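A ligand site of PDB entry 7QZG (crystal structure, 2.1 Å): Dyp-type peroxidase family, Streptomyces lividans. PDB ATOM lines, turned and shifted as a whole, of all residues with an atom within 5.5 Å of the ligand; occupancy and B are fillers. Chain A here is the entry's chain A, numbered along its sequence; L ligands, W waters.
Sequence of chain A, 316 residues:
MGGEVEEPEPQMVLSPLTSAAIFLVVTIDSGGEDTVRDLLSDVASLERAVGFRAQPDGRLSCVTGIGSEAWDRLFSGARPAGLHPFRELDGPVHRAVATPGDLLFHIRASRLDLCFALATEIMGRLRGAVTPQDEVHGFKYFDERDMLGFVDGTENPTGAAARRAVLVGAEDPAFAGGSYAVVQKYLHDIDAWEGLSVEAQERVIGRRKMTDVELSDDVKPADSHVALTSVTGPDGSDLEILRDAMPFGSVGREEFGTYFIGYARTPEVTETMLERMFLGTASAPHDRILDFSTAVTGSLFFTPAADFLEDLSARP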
ATOM      1  N   ASP A 146      25.650   2.832  18.939  1.00  0.00           N
ATOM      2  CA  ASP A 146      25.826   2.418  20.341  1.00  0.00           C
ATOM      3  C   ASP A 146      26.968   3.238  20.983  1.00  0.00           C
ATOM      4  O   ASP A 146      27.496   4.187  20.378  1.00  0.00           O
ATOM      5  CB  ASP A 146      26.081   0.906  20.401  1.00  0.00           C
ATOM      6  CG  ASP A 146      27.379   0.416  19.737  1.00  0.00           C
ATOM      7  OD1 ASP A 146      28.319   1.199  19.639  1.00  0.00           O
ATOM      8  OD2 ASP A 146      27.412  -0.759  19.345  1.00  0.00           O
ATOM      9  N   LEU A 148      30.016   2.626  21.594  1.00  0.00           N
ATOM     10  CA  LEU A 148      31.331   2.536  20.904  1.00  0.00           C
ATOM     11  C   LEU A 148      31.347   3.360  19.622  1.00  0.00           C
ATOM     12  O   LEU A 148      32.442   3.518  19.042  1.00  0.00           O
ATOM     13  CB  LEU A 148      31.678   1.074  20.647  1.00  0.00           C
ATOM     14  CG  LEU A 148      31.832   0.207  21.884  1.00  0.00           C
ATOM     15  CD1 LEU A 148      32.268  -1.197  21.526  1.00  0.00           C
ATOM     16  CD2 LEU A 148      32.829   0.842  22.862  1.00  0.00           C
ATOM     17  N   PHE A 150      29.586   2.749  16.846  1.00  0.00           N
ATOM     18  CA  PHE A 150      29.190   1.898  15.683  1.00  0.00           C
ATOM     19  C   PHE A 150      27.647   1.701  15.621  1.00  0.00           C
ATOM     20  O   PHE A 150      26.955   1.609  16.662  1.00  0.00           O
ATOM     21  CB  PHE A 150      29.884   0.552  15.780  1.00  0.00           C
ATOM     22  CG  PHE A 150      31.333   0.593  15.361  1.00  0.00           C
ATOM     23  CD1 PHE A 150      32.267   1.265  16.142  1.00  0.00           C
ATOM     24  CD2 PHE A 150      31.727   0.035  14.159  1.00  0.00           C
ATOM     25  CE1 PHE A 150      33.596   1.345  15.728  1.00  0.00           C
ATOM     26  CE2 PHE A 150      33.050   0.110  13.775  1.00  0.00           C
ATOM     27  CZ  PHE A 150      33.979   0.741  14.558  1.00  0.00           C
ATOM     28  N   VAL A 151      27.138   1.657  14.405  1.00  0.00           N
ATOM     29  CA  VAL A 151      25.724   1.252  14.155  1.00  0.00           C
ATOM     30  C   VAL A 151      25.518  -0.135  14.745  1.00  0.00           C
ATOM     31  O   VAL A 151      26.389  -1.035  14.573  1.00  0.00           O
ATOM     32  CB  VAL A 151      25.328   1.336  12.669  1.00  0.00           C
ATOM     33  CG1 VAL A 151      23.845   1.010  12.476  1.00  0.00           C
ATOM     34  CG2 VAL A 151      25.629   2.736  12.125  1.00  0.00           C
ATOM     35  N   ASP A 152      24.402  -0.278  15.456  1.00  0.00           N
ATOM     36  CA  ASP A 152      24.091  -1.456  16.267  1.00  0.00           C
ATOM     37  C   ASP A 152      22.679  -1.915  15.934  1.00  0.00           C
ATOM     38  O   ASP A 152      21.728  -1.200  16.363  1.00  0.00           O
ATOM     39  CB  ASP A 152      24.303  -1.090  17.737  1.00  0.00           C
ATOM     40  CG  ASP A 152      24.459  -2.294  18.637  1.00  0.00           C
ATOM     41  OD1 ASP A 152      23.730  -3.266  18.426  1.00  0.00           O
ATOM     42  OD2 ASP A 152      25.310  -2.217  19.549  1.00  0.00           O
ATOM     43  N   GLY A 153      22.555  -3.035  15.241  1.00  0.00           N
ATOM     44  CA  GLY A 153      21.243  -3.599  14.839  1.00  0.00           C
ATOM     45  C   GLY A 153      21.214  -4.100  13.429  1.00  0.00           C
ATOM     46  O   GLY A 153      20.333  -4.900  13.118  1.00  0.00           O
ATOM     47  N   THR A 154      22.195  -3.729  12.606  1.00  0.00           N
ATOM     48  CA  THR A 154      22.164  -3.808  11.123  1.00  0.00           C
ATOM     49  C   THR A 154      21.770  -5.186  10.657  1.00  0.00           C
ATOM     50  O   THR A 154      20.884  -5.257   9.768  1.00  0.00           O
ATOM     51  CB  THR A 154      23.532  -3.389  10.555  1.00  0.00           C
ATOM     52  OG1 THR A 154      23.866  -2.132  11.140  1.00  0.00           O
ATOM     53  CG2 THR A 154      23.518  -3.265   9.058  1.00  0.00           C
ATOM     54  N   GLU A 155      22.419  -6.247  11.178  1.00  0.00           N
ATOM     55  CA  GLU A 155      22.262  -7.617  10.613  1.00  0.00           C
ATOM     56  C   GLU A 155      21.218  -8.404  11.413  1.00  0.00           C
ATOM     57  O   GLU A 155      21.109  -9.624  11.153  1.00  0.00           O
ATOM     58  CB  GLU A 155      23.550  -8.391  10.568  1.00  0.00           C
ATOM     59  CG  GLU A 155      24.461  -7.899   9.466  1.00  0.00           C
ATOM     60  CD  GLU A 155      23.933  -8.081   8.070  1.00  0.00           C
ATOM     61  OE1 GLU A 155      23.957  -9.169   7.668  1.00  0.00           O
ATOM     62  OE2 GLU A 155      23.550  -7.096   7.362  1.00  0.00           O
ATOM     63  N   ASN A 156      20.400  -7.765  12.265  1.00  0.00           N
ATOM     64  CA  ASN A 156      19.241  -8.488  12.845  1.00  0.00           C
ATOM     65  C   ASN A 156      18.412  -9.079  11.710  1.00  0.00           C
ATOM     66  O   ASN A 156      18.263  -8.422  10.683  1.00  0.00           O
ATOM     67  CB  ASN A 156      18.353  -7.580  13.678  1.00  0.00           C
ATOM     68  CG  ASN A 156      18.746  -7.506  15.132  1.00  0.00           C
ATOM     69  OD1 ASN A 156      19.273  -8.477  15.669  1.00  0.00           O
ATOM     70  ND2 ASN A 156      18.519  -6.354  15.752  1.00  0.00           N
ATOM     71  N   GLN A 184      22.758  -9.051  29.513  1.00  0.00           N
ATOM     72  CA  GLN A 184      24.053  -8.707  30.158  1.00  0.00           C
ATOM     73  C   GLN A 184      24.215  -7.174  30.116  1.00  0.00           C
ATOM     74  O   GLN A 184      24.159  -6.583  29.013  1.00  0.00           O
ATOM     75  CB  GLN A 184      25.234  -9.323  29.409  1.00  0.00           C
ATOM     76  CG  GLN A 184      25.252 -10.855  29.396  1.00  0.00           C
ATOM     77  CD  GLN A 184      26.518 -11.296  28.624  1.00  0.00           C
ATOM     78  OE1 GLN A 184      26.697 -11.079  27.429  1.00  0.00           O
ATOM     79  NE2 GLN A 184      27.515 -11.804  29.330  1.00  0.00           N
ATOM     80  N   TYR A 186      26.857  -4.339  30.225  1.00  0.00           N
ATOM     81  CA  TYR A 186      28.290  -4.110  29.972  1.00  0.00           C
ATOM     82  C   TYR A 186      28.609  -2.640  30.333  1.00  0.00           C
ATOM     83  O   TYR A 186      27.859  -1.734  29.956  1.00  0.00           O
ATOM     84  CB  TYR A 186      28.636  -4.419  28.513  1.00  0.00           C
ATOM     85  CG  TYR A 186      28.727  -5.866  28.098  1.00  0.00           C
ATOM     86  CD1 TYR A 186      29.908  -6.589  28.198  1.00  0.00           C
ATOM     87  CD2 TYR A 186      27.607  -6.532  27.574  1.00  0.00           C
ATOM     88  CE1 TYR A 186      29.981  -7.922  27.841  1.00  0.00           C
ATOM     89  CE2 TYR A 186      27.681  -7.868  27.181  1.00  0.00           C
ATOM     90  CZ  TYR A 186      28.870  -8.561  27.310  1.00  0.00           C
ATOM     91  OH  TYR A 186      28.950  -9.895  26.837  1.00  0.00           O
ATOM     92  N   HIS A 188      31.796   0.049  29.452  1.00  0.00           N
ATOM     93  CA  HIS A 188      32.893   0.249  28.478  1.00  0.00           C
ATOM     94  C   HIS A 188      34.016   1.044  29.135  1.00  0.00           C
ATOM     95  O   HIS A 188      33.766   2.012  29.919  1.00  0.00           O
ATOM     96  CB  HIS A 188      32.400   0.881  27.165  1.00  0.00           C
ATOM     97  CG  HIS A 188      31.434   0.022  26.447  1.00  0.00           C
ATOM     98  ND1 HIS A 188      31.795  -1.226  25.920  1.00  0.00           N
ATOM     99  CD2 HIS A 188      30.107   0.196  26.214  1.00  0.00           C
ATOM    100  CE1 HIS A 188      30.719  -1.756  25.348  1.00  0.00           C
ATOM    101  NE2 HIS A 188      29.676  -0.900  25.512  1.00  0.00           N
ATOM    102  N   ILE A 205      35.585  -4.565  15.573  1.00  0.00           N
ATOM    103  CA  ILE A 205      34.153  -4.797  15.303  1.00  0.00           C
ATOM    104  C   ILE A 205      33.986  -5.747  14.094  1.00  0.00           C
ATOM    105  O   ILE A 205      33.230  -6.733  14.208  1.00  0.00           O
ATOM    106  CB  ILE A 205      33.379  -3.480  15.112  1.00  0.00           C
ATOM    107  CG1 ILE A 205      33.439  -2.635  16.368  1.00  0.00           C
ATOM    108  CG2 ILE A 205      31.926  -3.754  14.636  1.00  0.00           C
ATOM    109  CD1 ILE A 205      32.837  -3.290  17.581  1.00  0.00           C
ATOM    110  N   ARG A 207      33.410  -4.183  10.907  1.00  0.00           N
ATOM    111  CA  ARG A 207      32.610  -3.350   9.976  1.00  0.00           C
ATOM    112  C   ARG A 207      33.206  -1.940   9.951  1.00  0.00           C
ATOM    113  O   ARG A 207      33.856  -1.559  10.959  1.00  0.00           O
ATOM    114  CB  ARG A 207      31.118  -3.264  10.402  1.00  0.00           C
ATOM    115  CG  ARG A 207      30.396  -4.594  10.627  1.00  0.00           C
ATOM    116  CD  ARG A 207      28.934  -4.370  11.036  1.00  0.00           C
ATOM    117  NE  ARG A 207      28.159  -3.951   9.883  1.00  0.00           N
ATOM    118  CZ  ARG A 207      27.596  -4.754   8.982  1.00  0.00           C
ATOM    119  NH1 ARG A 207      27.552  -6.072   9.163  1.00  0.00           N
ATOM    120  NH2 ARG A 207      27.005  -4.200   7.934  1.00  0.00           N
ATOM    121  N   ASP A 212      29.243   1.661   7.839  1.00  0.00           N
ATOM    122  CA  ASP A 212      28.583   0.415   8.330  1.00  0.00           C
ATOM    123  C   ASP A 212      28.600  -0.665   7.231  1.00  0.00           C
ATOM    124  O   ASP A 212      27.745  -1.541   7.238  1.00  0.00           O
ATOM    125  CB  ASP A 212      27.142   0.652   8.778  1.00  0.00           C
ATOM    126  CG  ASP A 212      26.530  -0.440   9.625  1.00  0.00           C
ATOM    127  OD1 ASP A 212      27.316  -1.263  10.258  1.00  0.00           O
ATOM    128  OD2 ASP A 212      25.291  -0.459   9.691  1.00  0.00           O
ATOM    129  N   GLU A 214      30.333  -4.113   5.977  1.00  0.00           N
ATOM    130  CA  GLU A 214      31.128  -5.227   6.546  1.00  0.00           C
ATOM    131  C   GLU A 214      32.537  -5.273   5.881  1.00  0.00           C
ATOM    132  O   GLU A 214      32.613  -5.044   4.672  1.00  0.00           O
ATOM    133  CB  GLU A 214      30.360  -6.533   6.314  1.00  0.00           C
ATOM    134  CG  GLU A 214      30.948  -7.726   7.043  1.00  0.00           C
ATOM    135  CD  GLU A 214      30.156  -9.012   6.845  1.00  0.00           C
ATOM    136  OE1 GLU A 214      29.132  -9.028   6.032  1.00  0.00           O
ATOM    137  OE2 GLU A 214      30.611 -10.028   7.414  1.00  0.00           O
ATOM    138  N   HIS A 225      34.552  -9.066  16.475  1.00  0.00           N
ATOM    139  CA  HIS A 225      33.240  -9.327  17.071  1.00  0.00           C
ATOM    140  C   HIS A 225      32.315 -10.004  16.043  1.00  0.00           C
ATOM    141  O   HIS A 225      31.659 -11.025  16.371  1.00  0.00           O
ATOM    142  CB  HIS A 225      32.616  -8.044  17.589  1.00  0.00           C
ATOM    143  CG  HIS A 225      31.272  -8.262  18.215  1.00  0.00           C
ATOM    144  ND1 HIS A 225      31.105  -9.116  19.300  1.00  0.00           N
ATOM    145  CD2 HIS A 225      30.083  -7.694  17.966  1.00  0.00           C
ATOM    146  CE1 HIS A 225      29.844  -9.078  19.669  1.00  0.00           C
ATOM    147  NE2 HIS A 225      29.186  -8.215  18.848  1.00  0.00           N
ATOM    148  N   VAL A 226      32.291  -9.494  14.808  1.00  0.00           N
ATOM    149  CA  VAL A 226      31.344 -10.019  13.773  1.00  0.00           C
ATOM    150  C   VAL A 226      31.794 -11.442  13.352  1.00  0.00           C
ATOM    151  O   VAL A 226      30.918 -12.260  13.154  1.00  0.00           O
ATOM    152  CB  VAL A 226      31.220  -9.025  12.609  1.00  0.00           C
ATOM    153  CG1 VAL A 226      30.679  -9.693  11.343  1.00  0.00           C
ATOM    154  CG2 VAL A 226      30.328  -7.885  13.053  1.00  0.00           C
ATOM    155  N   THR A 229      30.611 -13.967  16.236  1.00  0.00           N
ATOM    156  CA  THR A 229      29.133 -14.075  16.468  1.00  0.00           C
ATOM    157  C   THR A 229      28.433 -14.571  15.206  1.00  0.00           C
ATOM    158  O   THR A 229      27.172 -14.595  15.166  1.00  0.00           O
ATOM    159  CB  THR A 229      28.577 -12.777  17.093  1.00  0.00           C
ATOM    160  OG1 THR A 229      28.909 -11.689  16.247  1.00  0.00           O
ATOM    161  CG2 THR A 229      29.110 -12.522  18.502  1.00  0.00           C
ATOM    162  N   SER A 230      29.208 -14.898  14.178  1.00  0.00           N
ATOM    163  CA  SER A 230      28.712 -15.508  12.910  1.00  0.00           C
ATOM    164  C   SER A 230      28.863 -17.018  13.046  1.00  0.00           C
ATOM    165  O   SER A 230      30.010 -17.451  13.199  1.00  0.00           O
ATOM    166  CB  SER A 230      29.458 -15.009  11.708  1.00  0.00           C
ATOM    167  OG  SER A 230      29.168 -13.637  11.484  1.00  0.00           O
ATOM    168  N   ILE A 241      20.107 -14.558  16.111  1.00  0.00           N
ATOM    169  CA  ILE A 241      19.331 -14.074  17.273  1.00  0.00           C
ATOM    170  C   ILE A 241      18.772 -12.687  16.886  1.00  0.00           C
ATOM    171  O   ILE A 241      19.279 -12.105  15.930  1.00  0.00           O
ATOM    172  CB  ILE A 241      20.215 -14.045  18.555  1.00  0.00           C
ATOM    173  CG1 ILE A 241      21.301 -12.953  18.487  1.00  0.00           C
ATOM    174  CG2 ILE A 241      20.757 -15.462  18.827  1.00  0.00           C
ATOM    175  CD1 ILE A 241      22.102 -12.821  19.712  1.00  0.00           C
ATOM    176  N   ARG A 243      18.563  -8.928  18.520  1.00  0.00           N
ATOM    177  CA  ARG A 243      19.129  -8.013  19.536  1.00  0.00           C
ATOM    178  C   ARG A 243      18.343  -6.710  19.617  1.00  0.00           C
ATOM    179  O   ARG A 243      17.839  -6.270  18.598  1.00  0.00           O
ATOM    180  CB  ARG A 243      20.572  -7.728  19.184  1.00  0.00           C
ATOM    181  CG  ARG A 243      21.460  -8.967  19.282  1.00  0.00           C
ATOM    182  CD  ARG A 243      22.792  -8.853  18.578  1.00  0.00           C
ATOM    183  NE  ARG A 243      22.739  -8.712  17.132  1.00  0.00           N
ATOM    184  CZ  ARG A 243      23.081  -7.616  16.435  1.00  0.00           C
ATOM    185  NH1 ARG A 243      23.614  -6.529  16.998  1.00  0.00           N
ATOM    186  NH2 ARG A 243      22.924  -7.600  15.135  1.00  0.00           N
ATOM    187  N   THR A 258      26.516  -0.489  27.646  1.00  0.00           N
ATOM    188  CA  THR A 258      25.594  -1.125  26.675  1.00  0.00           C
ATOM    189  C   THR A 258      24.789  -2.145  27.439  1.00  0.00           C
ATOM    190  O   THR A 258      25.423  -3.087  28.047  1.00  0.00           O
ATOM    191  CB  THR A 258      26.328  -1.829  25.532  1.00  0.00           C
ATOM    192  OG1 THR A 258      26.944  -0.789  24.805  1.00  0.00           O
ATOM    193  CG2 THR A 258      25.403  -2.597  24.603  1.00  0.00           C
ATOM    194  N   PHE A 260      22.833  -5.214  26.959  1.00  0.00           N
ATOM    195  CA  PHE A 260      22.594  -6.231  25.901  1.00  0.00           C
ATOM    196  C   PHE A 260      21.354  -7.060  26.244  1.00  0.00           C
ATOM    197  O   PHE A 260      21.293  -7.541  27.350  1.00  0.00           O
ATOM    198  CB  PHE A 260      23.835  -7.080  25.658  1.00  0.00           C
ATOM    199  CG  PHE A 260      23.592  -8.181  24.677  1.00  0.00           C
ATOM    200  CD1 PHE A 260      23.099  -9.393  25.101  1.00  0.00           C
ATOM    201  CD2 PHE A 260      23.817  -7.980  23.328  1.00  0.00           C
ATOM    202  CE1 PHE A 260      22.796 -10.401  24.186  1.00  0.00           C
ATOM    203  CE2 PHE A 260      23.577  -9.004  22.432  1.00  0.00           C
ATOM    204  CZ  PHE A 260      23.069 -10.204  22.854  1.00  0.00           C
ATOM    205  N   THR A 270      22.396 -18.603  21.563  1.00  0.00           N
ATOM    206  CA  THR A 270      23.003 -17.486  22.337  1.00  0.00           C
ATOM    207  C   THR A 270      24.238 -17.956  23.112  1.00  0.00           C
ATOM    208  O   THR A 270      25.257 -17.213  23.086  1.00  0.00           O
ATOM    209  CB  THR A 270      21.948 -16.825  23.231  1.00  0.00           C
ATOM    210  OG1 THR A 270      20.763 -16.704  22.428  1.00  0.00           O
ATOM    211  CG2 THR A 270      22.421 -15.475  23.717  1.00  0.00           C
ATOM    212  N   MET A 273      27.345 -18.459  20.900  1.00  0.00           N
ATOM    213  CA  MET A 273      27.927 -17.135  20.626  1.00  0.00           C
ATOM    214  C   MET A 273      28.750 -16.678  21.826  1.00  0.00           C
ATOM    215  O   MET A 273      29.919 -16.265  21.599  1.00  0.00           O
ATOM    216  CB  MET A 273      26.830 -16.122  20.262  1.00  0.00           C
ATOM    217  CG  MET A 273      26.324 -16.341  18.857  1.00  0.00           C
ATOM    218  SD  MET A 273      24.955 -15.250  18.606  1.00  0.00           S
ATOM    219  CE  MET A 273      24.384 -15.817  16.997  1.00  0.00           C
ATOM    220  N   LEU A 274      28.208 -16.743  23.049  1.00  0.00           N
ATOM    221  CA  LEU A 274      28.912 -16.292  24.291  1.00  0.00           C
ATOM    222  C   LEU A 274      30.186 -17.144  24.546  1.00  0.00           C
ATOM    223  O   LEU A 274      31.224 -16.537  24.829  1.00  0.00           O
ATOM    224  CB  LEU A 274      27.958 -16.386  25.482  1.00  0.00           C
ATOM    225  CG  LEU A 274      26.924 -15.260  25.553  1.00  0.00           C
ATOM    226  CD1 LEU A 274      25.846 -15.529  26.597  1.00  0.00           C
ATOM    227  CD2 LEU A 274      27.622 -13.941  25.869  1.00  0.00           C
ATOM    228  N   MET A 277      32.840 -15.954  22.206  1.00  0.00           N
ATOM    229  CA  MET A 277      33.311 -14.594  22.625  1.00  0.00           C
ATOM    230  C   MET A 277      34.268 -14.689  23.831  1.00  0.00           C
ATOM    231  O   MET A 277      35.329 -14.125  23.772  1.00  0.00           O
ATOM    232  CB  MET A 277      32.138 -13.664  22.982  1.00  0.00           C
ATOM    233  CG  MET A 277      31.304 -13.293  21.758  1.00  0.00           C
ATOM    234  SD  MET A 277      29.907 -12.293  22.364  1.00  0.00           S
ATOM    235  CE  MET A 277      30.709 -10.889  23.095  1.00  0.00           C
ATOM    236  N   ILE A 289      36.178  -7.200  21.286  1.00  0.00           N
ATOM    237  CA  ILE A 289      35.221  -6.231  21.918  1.00  0.00           C
ATOM    238  C   ILE A 289      35.334  -6.321  23.449  1.00  0.00           C
ATOM    239  O   ILE A 289      35.090  -5.305  24.128  1.00  0.00           O
ATOM    240  CB  ILE A 289      33.766  -6.410  21.415  1.00  0.00           C
ATOM    241  CG1 ILE A 289      32.988  -5.084  21.440  1.00  0.00           C
ATOM    242  CG2 ILE A 289      33.017  -7.473  22.183  1.00  0.00           C
ATOM    243  CD1 ILE A 289      31.607  -5.120  20.871  1.00  0.00           C
ATOM    244  N   SER A 293      35.053  -3.874  27.044  1.00  0.00           N
ATOM    245  CA  SER A 293      33.680  -4.104  27.581  1.00  0.00           C
ATOM    246  C   SER A 293      33.739  -5.119  28.720  1.00  0.00           C
ATOM    247  O   SER A 293      34.242  -6.228  28.483  1.00  0.00           O
ATOM    248  CB  SER A 293      32.708  -4.517  26.482  1.00  0.00           C
ATOM    249  OG  SER A 293      32.995  -3.895  25.265  1.00  0.00           O
HETATM  250  C1  LIG L   1      26.637  -7.495  15.631  1.00  0.00           C
HETATM  251  C2  LIG L   1      27.955  -4.272  19.185  1.00  0.00           C
HETATM  252  C3  LIG L   1      27.459  -7.728  22.539  1.00  0.00           C
HETATM  253  C4  LIG L   1      25.851 -10.815  19.059  1.00  0.00           C
HETATM  254  C5  LIG L   1      27.033  -6.362  16.337  1.00  0.00           C
HETATM  255  C6  LIG L   1      27.470  -5.186  15.730  1.00  0.00           C
HETATM  256  C7  LIG L   1      27.810  -4.258  16.694  1.00  0.00           C
HETATM  257  C8  LIG L   1      27.663  -4.878  17.911  1.00  0.00           C
HETATM  258  C9  LIG L   1      28.328  -2.867  16.448  1.00  0.00           C
HETATM  259  C10 LIG L   1      27.522  -4.995  14.198  1.00  0.00           C
HETATM  260  C11 LIG L   1      26.357  -4.309  13.531  1.00  0.00           C
HETATM  261  C12 LIG L   1      25.205  -5.323  13.597  1.00  0.00           C
HETATM  262  O1  LIG L   1      24.449  -5.240  14.564  1.00  0.00           O
HETATM  263  O2  LIG L   1      24.937  -6.308  12.826  1.00  0.00           O
HETATM  264  C13 LIG L   1      27.945  -4.959  20.416  1.00  0.00           C
HETATM  265  C14 LIG L   1      28.214  -4.315  21.700  1.00  0.00           C
HETATM  266  C15 LIG L   1      28.030  -5.251  22.644  1.00  0.00           C
HETATM  267  C16 LIG L   1      27.683  -6.519  21.918  1.00  0.00           C
HETATM  268  C17 LIG L   1      28.536  -2.856  22.092  1.00  0.00           C
HETATM  269  C18 LIG L   1      28.425  -4.898  24.019  1.00  0.00           C
HETATM  270  C19 LIG L   1      29.420  -5.553  24.559  1.00  0.00           C
HETATM  271  C20 LIG L   1      26.954  -8.885  21.871  1.00  0.00           C
HETATM  272  C21 LIG L   1      26.822 -10.175  22.455  1.00  0.00           C
HETATM  273  C22 LIG L   1      26.307 -11.038  21.474  1.00  0.00           C
HETATM  274  C23 LIG L   1      26.233 -10.295  20.247  1.00  0.00           C
HETATM  275  C24 LIG L   1      27.050 -10.432  23.943  1.00  0.00           C
HETATM  276  C25 LIG L   1      25.904 -12.469  21.571  1.00  0.00           C
HETATM  277  C26 LIG L   1      25.571 -13.060  22.677  1.00  0.00           C
HETATM  278  C27 LIG L   1      25.928 -10.136  17.888  1.00  0.00           C
HETATM  279  C28 LIG L   1      25.508 -10.727  16.638  1.00  0.00           C
HETATM  280  C29 LIG L   1      25.786  -9.818  15.660  1.00  0.00           C
HETATM  281  C30 LIG L   1      26.333  -8.655  16.337  1.00  0.00           C
HETATM  282  C31 LIG L   1      24.849 -12.032  16.285  1.00  0.00           C
HETATM  283  C32 LIG L   1      25.450 -10.051  14.190  1.00  0.00           C
HETATM  284  C33 LIG L   1      26.719 -10.644  13.536  1.00  0.00           C
HETATM  285  C34 LIG L   1      26.502 -10.982  12.089  1.00  0.00           C
HETATM  286  O3  LIG L   1      25.998 -12.024  11.855  1.00  0.00           O
HETATM  287  O4  LIG L   1      26.767 -10.308  11.089  1.00  0.00           O
HETATM  288  N1  LIG L   1      27.149  -6.147  17.695  1.00  0.00           N
HETATM  289  N2  LIG L   1      27.610  -6.261  20.603  1.00  0.00           N
HETATM  290  N3  LIG L   1      26.701  -8.999  20.527  1.00  0.00           N
HETATM  291  N4  LIG L   1      26.422  -8.854  17.711  1.00  0.00           N
HETATM  292 FE1  LIG L   1      27.193  -7.631  19.041  1.00  0.00          FE
HETATM  293  O   HOH W   1      24.462  -5.674  19.855  1.00  0.00           O
HETATM  294  O   HOH W   2      26.670 -10.407   8.681  1.00  0.00           O
HETATM  295  O   HOH W   3      24.924 -13.804  13.435  1.00  0.00           O
HETATM  296  O   HOH W   4      27.372  -7.502  11.922  1.00  0.00           O
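N of Glu 155 sits at hydrogen-bond distance from O2 of the ligand, at 3.0 Å. A ring nitrogen (NE2) of His 225 binds an iron atom (FE1) of the ligand. The backbone NH of Gly 153 is in hydrogen-bond range of an oxygen (O1) of the ligand (3.0 Å). NH2 of Arg 243 is in salt-bridge range of O1 of the ligand. N of Thr 154 is in hydrogen-bond range of O1 of the ligand (3.3 Å).
The side-chain hydroxyl of Ser 293 is in hydrogen-bond range of a ring nitrogen (ND1) of His 188 (3.0 Å). OG of Ser 230 lies within hydrogen-bond range of O of Val 226 (2.8 Å). The side-chain carboxylate of Asp 146 lies within hydrogen-bond range of the backbone NH of Phe 150 (3.4 Å). The backbone NH of Phe 260 is in hydrogen-bond range of the backbone carbonyl oxygen of Gln 184. The side-chain carboxylate (OD1) of Asp 146 lies within hydrogen-bond range of the backbone NH (N) of Leu 148, at 3.0 Å. The side-chain hydroxyl (OH) of Tyr 186 is in hydrogen-bond range of the side-chain amide oxygen (OE1) of Gln 184, at 2.6 Å. The side-chain amide nitrogen of Asn 156 is in hydrogen-bond range of the backbone carbonyl oxygen of Arg 243 (2.9 Å). N of Tyr 186 sits at hydrogen-bond distance from O of Thr 258 (2.9 Å).
Residues that only touch the ligand: Asp 146 (3.6 Å), Phe 150 (3.8 Å), Val 151 (3.3 Å), Asp 152 (3.4 Å), Gln 184 (3.6 Å), Tyr 186 (3.5 Å), Arg 207 (3.5 Å), Val 226 (3.97 Å), Thr 229 (3.6 Å), Ser 230 (3.6 Å), Thr 258 (3.8 Å), Phe 260 (3.4 Å), Met 273 (3.9 Å), Leu 274 (3.9 Å), Met 277 (3.7 Å), Ile 289 (3.6 Å) and Ser 293 (3.9 Å). Hydrophobic or aromatic side chains that line the ligand: Phe 150, Tyr 186, His 225, Val 226, Phe 260, Met 273, Leu 274, Met 277 and Ile 289. 22 residues have an atom within 4 Å of the ligand: Asp 146, Phe 150, Val 151, Asp 152, Gly 153, Thr 154, Glu 155, Gln 184, Tyr 186, Arg 207, His 225, Val 226, Thr 229, Ser 230, Arg 243, Thr 258, Phe 260, Met 273, Leu 274, Met 277, Ile 289 and Ser 293. Along chain A the residues within 4 Å of the ligand span positions 146 to 293. The nearest printed residue that does not touch the ligand is His 188 (4.1 Å).
Water W2 lies within hydrogen-bond range of O4 of the ligand (2.4 Å) and OE1 of Glu 155 (3.1 Å). Water W3 bridges an oxygen (O3) of the ligand (2.6 Å) and the backbone carbonyl oxygen (O) of Thr 229 (2.9 Å). Water W4 bridges O2 of the ligand (2.9 Å) and NH1 of Arg 207 (3.1 Å). Water W1 lies within hydrogen-bond range of OD1 of Asp 152 (2.9 Å) and NH1 of Arg 243 (3.1 Å).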
